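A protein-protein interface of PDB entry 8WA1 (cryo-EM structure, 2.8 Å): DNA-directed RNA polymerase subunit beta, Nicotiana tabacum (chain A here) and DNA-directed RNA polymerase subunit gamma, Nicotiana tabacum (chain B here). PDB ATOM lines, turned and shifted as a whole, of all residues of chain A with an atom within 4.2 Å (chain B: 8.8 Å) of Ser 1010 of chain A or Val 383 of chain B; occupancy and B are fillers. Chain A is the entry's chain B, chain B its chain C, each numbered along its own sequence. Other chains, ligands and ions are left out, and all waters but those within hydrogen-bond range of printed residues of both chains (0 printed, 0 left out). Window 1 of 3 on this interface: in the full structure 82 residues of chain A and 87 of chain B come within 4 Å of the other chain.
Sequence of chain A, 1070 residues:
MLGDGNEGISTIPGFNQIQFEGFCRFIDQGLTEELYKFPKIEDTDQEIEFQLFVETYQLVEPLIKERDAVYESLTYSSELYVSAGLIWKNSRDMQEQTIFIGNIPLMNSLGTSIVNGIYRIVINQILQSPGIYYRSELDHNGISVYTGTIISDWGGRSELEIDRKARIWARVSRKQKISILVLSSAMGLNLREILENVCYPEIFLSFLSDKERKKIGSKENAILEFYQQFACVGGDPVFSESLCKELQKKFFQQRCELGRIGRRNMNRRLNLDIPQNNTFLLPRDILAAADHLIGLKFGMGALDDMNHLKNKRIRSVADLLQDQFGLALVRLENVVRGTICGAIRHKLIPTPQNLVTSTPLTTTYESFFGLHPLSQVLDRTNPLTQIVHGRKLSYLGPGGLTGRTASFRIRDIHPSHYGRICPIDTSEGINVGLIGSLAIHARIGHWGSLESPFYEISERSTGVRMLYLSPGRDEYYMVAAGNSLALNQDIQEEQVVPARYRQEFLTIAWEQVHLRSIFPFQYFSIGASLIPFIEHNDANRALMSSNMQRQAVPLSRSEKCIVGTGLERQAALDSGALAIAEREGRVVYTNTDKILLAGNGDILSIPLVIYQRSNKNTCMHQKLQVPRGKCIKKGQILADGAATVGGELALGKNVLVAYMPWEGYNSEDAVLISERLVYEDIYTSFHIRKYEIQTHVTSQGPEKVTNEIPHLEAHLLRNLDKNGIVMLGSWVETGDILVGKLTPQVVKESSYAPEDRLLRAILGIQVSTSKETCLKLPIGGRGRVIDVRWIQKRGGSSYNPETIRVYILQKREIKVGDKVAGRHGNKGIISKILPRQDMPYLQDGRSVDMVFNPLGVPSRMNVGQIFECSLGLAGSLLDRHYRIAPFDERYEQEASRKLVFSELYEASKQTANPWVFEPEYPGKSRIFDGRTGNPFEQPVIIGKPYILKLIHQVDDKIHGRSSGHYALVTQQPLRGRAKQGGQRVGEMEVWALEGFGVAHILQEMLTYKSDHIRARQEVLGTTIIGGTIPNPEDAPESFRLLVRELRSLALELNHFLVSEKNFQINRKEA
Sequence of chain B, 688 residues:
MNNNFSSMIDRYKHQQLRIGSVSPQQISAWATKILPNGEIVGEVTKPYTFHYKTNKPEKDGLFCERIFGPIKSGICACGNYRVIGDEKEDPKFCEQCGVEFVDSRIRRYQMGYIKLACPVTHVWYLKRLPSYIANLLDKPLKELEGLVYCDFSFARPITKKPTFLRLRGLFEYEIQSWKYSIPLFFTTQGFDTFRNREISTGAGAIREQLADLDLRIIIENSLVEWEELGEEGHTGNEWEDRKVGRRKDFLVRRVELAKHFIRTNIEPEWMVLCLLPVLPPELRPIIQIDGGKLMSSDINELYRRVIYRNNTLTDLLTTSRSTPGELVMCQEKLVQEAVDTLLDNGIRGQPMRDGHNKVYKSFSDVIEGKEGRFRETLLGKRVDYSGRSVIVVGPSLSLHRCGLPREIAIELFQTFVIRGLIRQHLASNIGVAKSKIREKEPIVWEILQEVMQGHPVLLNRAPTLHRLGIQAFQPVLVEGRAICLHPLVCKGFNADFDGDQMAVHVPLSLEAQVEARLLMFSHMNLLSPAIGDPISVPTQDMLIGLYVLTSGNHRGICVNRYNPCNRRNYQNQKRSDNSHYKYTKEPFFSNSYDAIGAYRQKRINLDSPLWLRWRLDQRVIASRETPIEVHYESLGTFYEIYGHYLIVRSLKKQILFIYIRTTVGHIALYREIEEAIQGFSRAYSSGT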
ATOM      1  N   GLN A 971      13.642 -18.590  16.997  1.00  0.00           N
ATOM      2  CA  GLN A 971      15.099 -18.530  17.072  1.00  0.00           C
ATOM      3  C   GLN A 971      15.734 -18.839  15.754  1.00  0.00           C
ATOM      4  O   GLN A 971      16.932 -19.042  15.675  1.00  0.00           O
ATOM      5  CB  GLN A 971      15.677 -19.335  18.222  1.00  0.00           C
ATOM      6  CG  GLN A 971      15.377 -18.725  19.571  1.00  0.00           C
ATOM      7  CD  GLN A 971      16.160 -17.462  19.834  1.00  0.00           C
ATOM      8  OE1 GLN A 971      17.286 -17.308  19.373  1.00  0.00           O
ATOM      9  NE2 GLN A 971      15.571 -16.554  20.593  1.00  0.00           N
ATOM     10  N   GLN A 972      14.936 -18.865  14.705  1.00  0.00           N
ATOM     11  CA  GLN A 972      15.461 -19.069  13.379  1.00  0.00           C
ATOM     12  C   GLN A 972      15.933 -17.726  12.917  1.00  0.00           C
ATOM     13  O   GLN A 972      15.593 -16.722  13.515  1.00  0.00           O
ATOM     14  CB  GLN A 972      14.373 -19.577  12.455  1.00  0.00           C
ATOM     15  CG  GLN A 972      13.625 -20.781  12.965  1.00  0.00           C
ATOM     16  CD  GLN A 972      12.857 -21.491  11.877  1.00  0.00           C
ATOM     17  OE1 GLN A 972      12.724 -20.983  10.767  1.00  0.00           O
ATOM     18  NE2 GLN A 972      12.344 -22.670  12.192  1.00  0.00           N
ATOM     19  N   PRO A 973      16.698 -17.678  11.834  1.00  0.00           N
ATOM     20  CA  PRO A 973      17.069 -16.362  11.336  1.00  0.00           C
ATOM     21  C   PRO A 973      15.869 -15.560  10.846  1.00  0.00           C
ATOM     22  O   PRO A 973      14.853 -16.144  10.511  1.00  0.00           O
ATOM     23  CB  PRO A 973      17.987 -16.693  10.178  1.00  0.00           C
ATOM     24  CG  PRO A 973      18.587 -17.999  10.538  1.00  0.00           C
ATOM     25  CD  PRO A 973      17.469 -18.745  11.182  1.00  0.00           C
ATOM     26  N   GLY A 982      18.418 -14.450   6.180  1.00  0.00           N
ATOM     27  CA  GLY A 982      18.876 -15.439   5.230  1.00  0.00           C
ATOM     28  C   GLY A 982      17.758 -15.933   4.331  1.00  0.00           C
ATOM     29  O   GLY A 982      16.635 -15.428   4.334  1.00  0.00           O
ATOM     30  N   GLN A 983      18.087 -16.954   3.547  1.00  0.00           N
ATOM     31  CA  GLN A 983      17.151 -17.570   2.621  1.00  0.00           C
ATOM     32  C   GLN A 983      16.563 -18.830   3.242  1.00  0.00           C
ATOM     33  O   GLN A 983      17.149 -19.447   4.135  1.00  0.00           O
ATOM     34  CB  GLN A 983      17.836 -17.896   1.287  1.00  0.00           C
ATOM     35  CG  GLN A 983      18.539 -16.709   0.645  1.00  0.00           C
ATOM     36  CD  GLN A 983      17.601 -15.550   0.371  1.00  0.00           C
ATOM     37  OE1 GLN A 983      16.451 -15.744  -0.025  1.00  0.00           O
ATOM     38  NE2 GLN A 983      18.089 -14.333   0.583  1.00  0.00           N
ATOM     39  N   VAL A 985      15.047 -22.677   3.263  1.00  0.00           N
ATOM     40  CA  VAL A 985      15.142 -24.013   2.690  1.00  0.00           C
ATOM     41  C   VAL A 985      13.799 -24.692   2.920  1.00  0.00           C
ATOM     42  O   VAL A 985      13.525 -25.187   4.020  1.00  0.00           O
ATOM     43  CB  VAL A 985      16.289 -24.823   3.305  1.00  0.00           C
ATOM     44  CG1 VAL A 985      16.398 -26.182   2.632  1.00  0.00           C
ATOM     45  CG2 VAL A 985      17.599 -24.059   3.192  1.00  0.00           C
ATOM     46  N   MET A1005      22.280 -27.533   7.857  1.00  0.00           N
ATOM     47  CA  MET A1005      21.324 -26.470   7.565  1.00  0.00           C
ATOM     48  C   MET A1005      20.145 -26.501   8.528  1.00  0.00           C
ATOM     49  O   MET A1005      19.622 -25.449   8.911  1.00  0.00           O
ATOM     50  CB  MET A1005      20.830 -26.589   6.123  1.00  0.00           C
ATOM     51  CG  MET A1005      21.885 -26.303   5.070  1.00  0.00           C
ATOM     52  SD  MET A1005      21.214 -26.353   3.398  1.00  0.00           S
ATOM     53  CE  MET A1005      22.639 -25.837   2.446  1.00  0.00           C
ATOM     54  N   THR A1007      20.226 -27.655  11.644  1.00  0.00           N
ATOM     55  CA  THR A1007      20.533 -27.434  13.050  1.00  0.00           C
ATOM     56  C   THR A1007      21.327 -26.158  13.311  1.00  0.00           C
ATOM     57  O   THR A1007      20.801 -25.241  13.950  1.00  0.00           O
ATOM     58  CB  THR A1007      21.296 -28.634  13.619  1.00  0.00           C
ATOM     59  OG1 THR A1007      22.497 -28.846  12.868  1.00  0.00           O
ATOM     60  CG2 THR A1007      20.437 -29.888  13.558  1.00  0.00           C
ATOM     61  N   TYR A1008      22.541 -26.026  12.765  1.00  0.00           N
ATOM     62  CA  TYR A1008      23.406 -24.985  13.320  1.00  0.00           C
ATOM     63  C   TYR A1008      23.410 -23.728  12.460  1.00  0.00           C
ATOM     64  O   TYR A1008      23.731 -22.640  12.950  1.00  0.00           O
ATOM     65  CB  TYR A1008      24.827 -25.510  13.571  1.00  0.00           C
ATOM     66  CG  TYR A1008      25.691 -25.913  12.394  1.00  0.00           C
ATOM     67  CD1 TYR A1008      26.109 -24.986  11.447  1.00  0.00           C
ATOM     68  CD2 TYR A1008      26.152 -27.218  12.274  1.00  0.00           C
ATOM     69  CE1 TYR A1008      26.922 -25.358  10.390  1.00  0.00           C
ATOM     70  CE2 TYR A1008      26.970 -27.596  11.230  1.00  0.00           C
ATOM     71  CZ  TYR A1008      27.350 -26.663  10.289  1.00  0.00           C
ATOM     72  OH  TYR A1008      28.159 -27.041   9.244  1.00  0.00           O
ATOM     73  N   LYS A1009      23.056 -23.848  11.183  1.00  0.00           N
ATOM     74  CA  LYS A1009      22.838 -22.639  10.402  1.00  0.00           C
ATOM     75  C   LYS A1009      21.467 -22.028  10.655  1.00  0.00           C
ATOM     76  O   LYS A1009      21.223 -20.898  10.221  1.00  0.00           O
ATOM     77  CB  LYS A1009      23.018 -22.924   8.910  1.00  0.00           C
ATOM     78  CG  LYS A1009      24.420 -23.387   8.543  1.00  0.00           C
ATOM     79  CD  LYS A1009      24.810 -22.946   7.139  1.00  0.00           C
ATOM     80  CE  LYS A1009      23.853 -23.484   6.090  1.00  0.00           C
ATOM     81  NZ  LYS A1009      24.248 -23.070   4.714  1.00  0.00           N
ATOM     82  N   SER A1010      20.570 -22.744  11.331  1.00  0.00           N
ATOM     83  CA  SER A1010      19.216 -22.244  11.516  1.00  0.00           C
ATOM     84  C   SER A1010      18.841 -21.993  12.973  1.00  0.00           C
ATOM     85  O   SER A1010      18.500 -20.864  13.336  1.00  0.00           O
ATOM     86  CB  SER A1010      18.216 -23.222  10.902  1.00  0.00           C
ATOM     87  OG  SER A1010      18.547 -23.511   9.557  1.00  0.00           O
ATOM     88  N   ASP A1011      18.912 -23.019  13.822  1.00  0.00           N
ATOM     89  CA  ASP A1011      18.193 -22.981  15.086  1.00  0.00           C
ATOM     90  C   ASP A1011      19.031 -23.371  16.297  1.00  0.00           C
ATOM     91  O   ASP A1011      18.683 -22.984  17.417  1.00  0.00           O
ATOM     92  CB  ASP A1011      16.967 -23.893  15.012  1.00  0.00           C
ATOM     93  CG  ASP A1011      15.681 -23.162  15.319  1.00  0.00           C
ATOM     94  OD1 ASP A1011      15.555 -22.632  16.439  1.00  0.00           O
ATOM     95  OD2 ASP A1011      14.803 -23.102  14.434  1.00  0.00           O
ATOM     96  N   HIS A1012      20.121 -24.110  16.117  1.00  0.00           N
ATOM     97  CA  HIS A1012      20.856 -24.660  17.252  1.00  0.00           C
ATOM     98  C   HIS A1012      21.701 -23.549  17.861  1.00  0.00           C
ATOM     99  O   HIS A1012      22.751 -23.190  17.321  1.00  0.00           O
ATOM    100  CB  HIS A1012      21.716 -25.848  16.830  1.00  0.00           C
ATOM    101  CG  HIS A1012      21.909 -26.863  17.914  1.00  0.00           C
ATOM    102  ND1 HIS A1012      22.661 -28.005  17.738  1.00  0.00           N
ATOM    103  CD2 HIS A1012      21.444 -26.911  19.184  1.00  0.00           C
ATOM    104  CE1 HIS A1012      22.653 -28.711  18.854  1.00  0.00           C
ATOM    105  NE2 HIS A1012      21.921 -28.070  19.747  1.00  0.00           N
ATOM    106  N   ARG A1016      25.499 -22.906  17.035  1.00  0.00           N
ATOM    107  CA  ARG A1016      25.766 -21.712  16.258  1.00  0.00           C
ATOM    108  C   ARG A1016      26.767 -20.827  16.953  1.00  0.00           C
ATOM    109  O   ARG A1016      27.617 -20.225  16.315  1.00  0.00           O
ATOM    110  CB  ARG A1016      24.495 -20.987  15.813  1.00  0.00           C
ATOM    111  CG  ARG A1016      23.803 -20.072  16.790  1.00  0.00           C
ATOM    112  CD  ARG A1016      22.386 -19.865  16.298  1.00  0.00           C
ATOM    113  NE  ARG A1016      21.561 -19.140  17.248  1.00  0.00           N
ATOM    114  CZ  ARG A1016      20.240 -19.077  17.165  1.00  0.00           C
ATOM    115  NH1 ARG A1016      19.615 -19.708  16.184  1.00  0.00           N
ATOM    116  NH2 ARG A1016      19.549 -18.397  18.060  1.00  0.00           N
ATOM    117  N   THR B 377       7.823 -24.682  10.586  1.00  0.00           N
ATOM    118  CA  THR B 377       9.061 -24.648  11.359  1.00  0.00           C
ATOM    119  C   THR B 377       9.924 -25.893  11.183  1.00  0.00           C
ATOM    120  O   THR B 377      11.097 -25.782  10.816  1.00  0.00           O
ATOM    121  CB  THR B 377       8.748 -24.449  12.846  1.00  0.00           C
ATOM    122  OG1 THR B 377       7.997 -25.567  13.335  1.00  0.00           O
ATOM    123  CG2 THR B 377       7.945 -23.175  13.054  1.00  0.00           C
ATOM    124  N   LEU B 378       9.370 -27.082  11.436  1.00  0.00           N
ATOM    125  CA  LEU B 378      10.202 -28.279  11.521  1.00  0.00           C
ATOM    126  C   LEU B 378      10.670 -28.734  10.144  1.00  0.00           C
ATOM    127  O   LEU B 378      11.853 -29.041   9.954  1.00  0.00           O
ATOM    128  CB  LEU B 378       9.429 -29.398  12.216  1.00  0.00           C
ATOM    129  CG  LEU B 378       8.899 -29.096  13.617  1.00  0.00           C
ATOM    130  CD1 LEU B 378       7.857 -30.121  14.019  1.00  0.00           C
ATOM    131  CD2 LEU B 378      10.038 -29.070  14.620  1.00  0.00           C
ATOM    132  N   GLY B 380      10.532 -26.924   7.330  1.00  0.00           N
ATOM    133  CA  GLY B 380      11.052 -25.837   6.528  1.00  0.00           C
ATOM    134  C   GLY B 380      11.584 -24.710   7.385  1.00  0.00           C
ATOM    135  O   GLY B 380      10.910 -24.265   8.319  1.00  0.00           O
ATOM    136  N   LYS B 381      12.792 -24.238   7.085  1.00  0.00           N
ATOM    137  CA  LYS B 381      13.406 -23.188   7.881  1.00  0.00           C
ATOM    138  C   LYS B 381      14.441 -22.458   7.041  1.00  0.00           C
ATOM    139  O   LYS B 381      14.906 -22.960   6.015  1.00  0.00           O
ATOM    140  CB  LYS B 381      14.046 -23.755   9.155  1.00  0.00           C
ATOM    141  CG  LYS B 381      14.981 -24.928   8.912  1.00  0.00           C
ATOM    142  CD  LYS B 381      15.456 -25.530  10.225  1.00  0.00           C
ATOM    143  CE  LYS B 381      14.282 -25.991  11.074  1.00  0.00           C
ATOM    144  NZ  LYS B 381      14.721 -26.543  12.384  1.00  0.00           N
ATOM    145  N   ARG B 382      14.794 -21.261   7.493  1.00  0.00           N
ATOM    146  CA  ARG B 382      15.811 -20.448   6.846  1.00  0.00           C
ATOM    147  C   ARG B 382      17.148 -20.624   7.556  1.00  0.00           C
ATOM    148  O   ARG B 382      17.203 -20.887   8.759  1.00  0.00           O
ATOM    149  CB  ARG B 382      15.399 -18.973   6.831  1.00  0.00           C
ATOM    150  CG  ARG B 382      14.851 -18.465   8.150  1.00  0.00           C
ATOM    151  CD  ARG B 382      13.597 -17.619   7.950  1.00  0.00           C
ATOM    152  NE  ARG B 382      13.811 -16.507   7.028  1.00  0.00           N
ATOM    153  CZ  ARG B 382      13.281 -16.431   5.810  1.00  0.00           C
ATOM    154  NH1 ARG B 382      12.497 -17.403   5.366  1.00  0.00           N
ATOM    155  NH2 ARG B 382      13.530 -15.382   5.038  1.00  0.00           N
ATOM    156  N   VAL B 383      18.211 -20.333   6.824  1.00  0.00           N
ATOM    157  CA  VAL B 383      19.527 -20.528   7.359  1.00  0.00           C
ATOM    158  C   VAL B 383      20.388 -19.301   7.338  1.00  0.00           C
ATOM    159  O   VAL B 383      20.062 -18.324   6.687  1.00  0.00           O
ATOM    160  CB  VAL B 383      20.238 -21.560   6.496  1.00  0.00           C
ATOM    161  CG1 VAL B 383      19.533 -22.898   6.568  1.00  0.00           C
ATOM    162  CG2 VAL B 383      20.293 -21.097   5.053  1.00  0.00           C
ATOM    163  N   ASP B 384      21.482 -19.331   8.078  1.00  0.00           N
ATOM    164  CA  ASP B 384      22.440 -18.252   8.065  1.00  0.00           C
ATOM    165  C   ASP B 384      23.304 -18.541   6.892  1.00  0.00           C
ATOM    166  O   ASP B 384      23.174 -19.586   6.283  1.00  0.00           O
ATOM    167  CB  ASP B 384      23.309 -18.304   9.297  1.00  0.00           C
ATOM    168  CG  ASP B 384      22.609 -17.811  10.528  1.00  0.00           C
ATOM    169  OD1 ASP B 384      21.790 -16.882  10.415  1.00  0.00           O
ATOM    170  OD2 ASP B 384      22.896 -18.341  11.616  1.00  0.00           O
ATOM    171  N   TYR B 385      24.185 -17.623   6.556  1.00  0.00           N
ATOM    172  CA  TYR B 385      25.051 -17.789   5.406  1.00  0.00           C
ATOM    173  C   TYR B 385      24.240 -17.999   4.147  1.00  0.00           C
ATOM    174  O   TYR B 385      24.347 -19.036   3.516  1.00  0.00           O
ATOM    175  CB  TYR B 385      26.040 -18.921   5.625  1.00  0.00           C
ATOM    176  CG  TYR B 385      26.845 -18.757   6.885  1.00  0.00           C
ATOM    177  CD1 TYR B 385      27.916 -17.885   6.932  1.00  0.00           C
ATOM    178  CD2 TYR B 385      26.524 -19.461   8.032  1.00  0.00           C
ATOM    179  CE1 TYR B 385      28.651 -17.724   8.086  1.00  0.00           C
ATOM    180  CE2 TYR B 385      27.250 -19.305   9.190  1.00  0.00           C
ATOM    181  CZ  TYR B 385      28.312 -18.438   9.209  1.00  0.00           C
ATOM    182  OH  TYR B 385      29.037 -18.283  10.361  1.00  0.00           O
ATOM    183  N   SER B 386      23.434 -17.005   3.778  1.00  0.00           N
ATOM    184  CA  SER B 386      22.627 -17.125   2.575  1.00  0.00           C
ATOM    185  C   SER B 386      22.450 -15.757   1.931  1.00  0.00           C
ATOM    186  O   SER B 386      22.408 -14.731   2.614  1.00  0.00           O
ATOM    187  CB  SER B 386      21.254 -17.743   2.875  1.00  0.00           C
ATOM    188  N   GLY B 387      22.349 -15.758   0.604  1.00  0.00           N
ATOM    189  CA  GLY B 387      22.135 -14.531  -0.141  1.00  0.00           C
ATOM    190  C   GLY B 387      21.437 -14.820  -1.451  1.00  0.00           C
ATOM    191  O   GLY B 387      21.574 -15.902  -2.028  1.00  0.00           O
ATOM    192  N   LEU B 412      29.132 -13.651   2.895  1.00  0.00           N
ATOM    193  CA  LEU B 412      29.030 -15.090   3.114  1.00  0.00           C
ATOM    194  C   LEU B 412      30.287 -15.640   3.778  1.00  0.00           C
ATOM    195  O   LEU B 412      30.202 -16.384   4.761  1.00  0.00           O
ATOM    196  CB  LEU B 412      28.764 -15.811   1.795  1.00  0.00           C
ATOM    197  CG  LEU B 412      27.451 -15.482   1.084  1.00  0.00           C
ATOM    198  CD1 LEU B 412      27.287 -16.351  -0.148  1.00  0.00           C
ATOM    199  CD2 LEU B 412      26.274 -15.650   2.025  1.00  0.00           C
ATOM    200  N   ASN B 460      20.580 -22.587  -5.588  1.00  0.00           N
ATOM    201  CA  ASN B 460      19.257 -23.194  -5.608  1.00  0.00           C
ATOM    202  C   ASN B 460      18.237 -22.171  -6.088  1.00  0.00           C
ATOM    203  O   ASN B 460      18.492 -20.966  -6.098  1.00  0.00           O
ATOM    204  CB  ASN B 460      18.862 -23.734  -4.229  1.00  0.00           C
ATOM    205  CG  ASN B 460      18.804 -22.651  -3.175  1.00  0.00           C
ATOM    206  OD1 ASN B 460      19.829 -22.256  -2.618  1.00  0.00           O
ATOM    207  ND2 ASN B 460      17.602 -22.165  -2.892  1.00  0.00           N
ATOM    208  N   ALA B 503      19.386 -18.433  -4.765  1.00  0.00           N
ATOM    209  CA  ALA B 503      20.005 -18.359  -3.470  1.00  0.00           C
ATOM    210  C   ALA B 503      21.370 -18.992  -3.417  1.00  0.00           C
ATOM    211  O   ALA B 503      21.707 -19.748  -4.303  1.00  0.00           O
ATOM    212  CB  ALA B 503      19.112 -18.994  -2.463  1.00  0.00           C
ATOM    213  N   VAL B 504      22.148 -18.725  -2.379  1.00  0.00           N
ATOM    214  CA  VAL B 504      23.519 -19.206  -2.235  1.00  0.00           C
ATOM    215  C   VAL B 504      23.681 -19.769  -0.831  1.00  0.00           C
ATOM    216  O   VAL B 504      23.165 -19.196   0.134  1.00  0.00           O
ATOM    217  CB  VAL B 504      24.553 -18.088  -2.484  1.00  0.00           C
ATOM    218  CG1 VAL B 504      25.955 -18.665  -2.533  1.00  0.00           C
ATOM    219  CG2 VAL B 504      24.241 -17.329  -3.767  1.00  0.00           C
ATOM    220  N   HIS B 505      24.403 -20.884  -0.711  1.00  0.00           N
ATOM    221  CA  HIS B 505      24.639 -21.525   0.575  1.00  0.00           C
ATOM    222  C   HIS B 505      26.085 -21.990   0.667  1.00  0.00           C
ATOM    223  O   HIS B 505      26.635 -22.534  -0.296  1.00  0.00           O
ATOM    224  CB  HIS B 505      23.693 -22.712   0.788  1.00  0.00           C
ATOM    225  CG  HIS B 505      22.256 -22.320   0.920  1.00  0.00           C
ATOM    226  ND1 HIS B 505      21.249 -22.930   0.203  1.00  0.00           N
ATOM    227  CD2 HIS B 505      21.655 -21.382   1.689  1.00  0.00           C
ATOM    228  CE1 HIS B 505      20.091 -22.382   0.523  1.00  0.00           C
ATOM    229  NE2 HIS B 505      20.309 -21.440   1.423  1.00  0.00           N
ATOM    230  N   VAL B 506      26.688 -21.783   1.828  1.00  0.00           N
ATOM    231  CA  VAL B 506      28.098 -22.090   2.063  1.00  0.00           C
ATOM    232  C   VAL B 506      28.188 -23.247   3.053  1.00  0.00           C
ATOM    233  O   VAL B 506      27.736 -23.100   4.197  1.00  0.00           O
ATOM    234  CB  VAL B 506      28.859 -20.861   2.593  1.00  0.00           C
ATOM    235  CG1 VAL B 506      30.316 -21.204   2.849  1.00  0.00           C
ATOM    236  CG2 VAL B 506      28.741 -19.700   1.616  1.00  0.00           C
ATOM    237  N   LEU B 508      29.797 -25.240   5.893  1.00  0.00           N
ATOM    238  CA  LEU B 508      30.821 -24.955   6.895  1.00  0.00           C
ATOM    239  C   LEU B 508      31.644 -26.195   7.227  1.00  0.00           C
ATOM    240  O   LEU B 508      32.879 -26.136   7.255  1.00  0.00           O
ATOM    241  CB  LEU B 508      30.175 -24.393   8.162  1.00  0.00           C
ATOM    242  CG  LEU B 508      29.918 -22.886   8.260  1.00  0.00           C
ATOM    243  CD1 LEU B 508      31.228 -22.121   8.162  1.00  0.00           C
ATOM    244  CD2 LEU B 508      28.930 -22.404   7.207  1.00  0.00           C
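The side-chain hydroxyl of Ser 1010 of chain A lies within hydrogen-bond range of the backbone carbonyl oxygen of Arg 382 of chain B, 3.1 Å away. The backbone carbonyl oxygen (O) of Lys 381 of chain B sits at hydrogen-bond distance from the backbone NH (N) of Val 985 of chain A, at 2.8 Å. The guanidinium group (NH2) of Arg 382 of chain B lies within hydrogen-bond range of the backbone carbonyl oxygen (O) of Gly 982 of chain A, 3.2 Å away. The backbone carbonyl oxygen (O) of Gln 983 of chain A is in hydrogen-bond range of the backbone NH (N) of Val 383 of chain B. The backbone carbonyl oxygen (O) of Lys 1009 of chain A lies within hydrogen-bond range of the backbone NH (N) of Asp 384 of chain B, 2.7 Å away.
OD1 of Asn 460 of chain B lies close to ND1 of His 505 of chain B, 3.2 Å away. The side-chain amide nitrogen (NE2) of Gln 972 of chain A lies close to the side-chain carboxylate (OD2) of Asp 1011 of chain A. The backbone carbonyl oxygen of Ser 1010 of chain A lies within hydrogen-bond range of the guanidinium group of Arg 1016 of chain A. N of Ala 503 of chain B lies within hydrogen-bond range of O of Asn 460 of chain B. O of Gly 387 of chain B lies within hydrogen-bond range of N of Val 504 of chain B, at 2.9 Å.
Gln 972 of chain A touches Thr 377 of chain B (NE2 to O, 3.6 Å). Gln 972 of chain A touches Arg 382 of chain B. CD of Arg 382 of chain B touches O of Pro 973 of chain A (3.2 Å). Asp 384 of chain B touches Pro 973 of chain A. O of Val 383 of chain B touches CA of Gly 982 of chain A, at 3.4 Å. Gln 983 of chain A touches Ser 386 of chain B (N to CB, 3.3 Å). Gln 983 of chain A touches Ala 503 of chain B. Val 985 of chain A touches Gly 380 of chain B. Lys 1009 of chain A touches Tyr 385 of chain B (CD to CD2, 3.99 Å). Val 383 of chain B touches Ser 1010 of chain A (CG1 to OG, 3.2 Å).
Printed residues of chain A within 4 Å of Ala 503 of chain B: Gln 983. Of the printed residues of chain B, Gln 972 of chain A touches Thr 377 (3.6 Å), Lys 381 (3.5 Å) and Arg 382 (3.9 Å). Of the printed residues of chain B, Pro 973 of chain A touches Arg 382 (3.2 Å), Val 383 (3.9 Å) and Asp 384 (3.4 Å). Printed residues of chain B within 4 Å of Lys 1009 of chain A: Val 383 (3.3 Å), Asp 384 (2.7 Å), Tyr 385 (3.99 Å), His 505 (3.98 Å) and Val 506 (3.5 Å). Of the printed residues of chain A, Tyr 385 of chain B touches Lys 1009 (3.99 Å). The nearest residue of chain A that does not touch Val 383 of chain B is Val 985 of chain A (4.1 Å).
Printed residues of chain A that touch a printed residue of chain B: Gln 972, Pro 973, Gly 982, Gln 983, Val 985, Met 1005, Tyr 1008, Lys 1009 and Ser 1010. Hydrophobic or aromatic side chains of chain A that line the printed part of chain B: Pro 973, Val 985, Met 1005 and Tyr 1008. Hydrophobic or aromatic side chains of chain B within 4 Å of the printed part of chain A: Val 383, Tyr 385, Ala 503, His 505 and Leu 508. Among the printed residues, 26 pairs touch across the chains.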
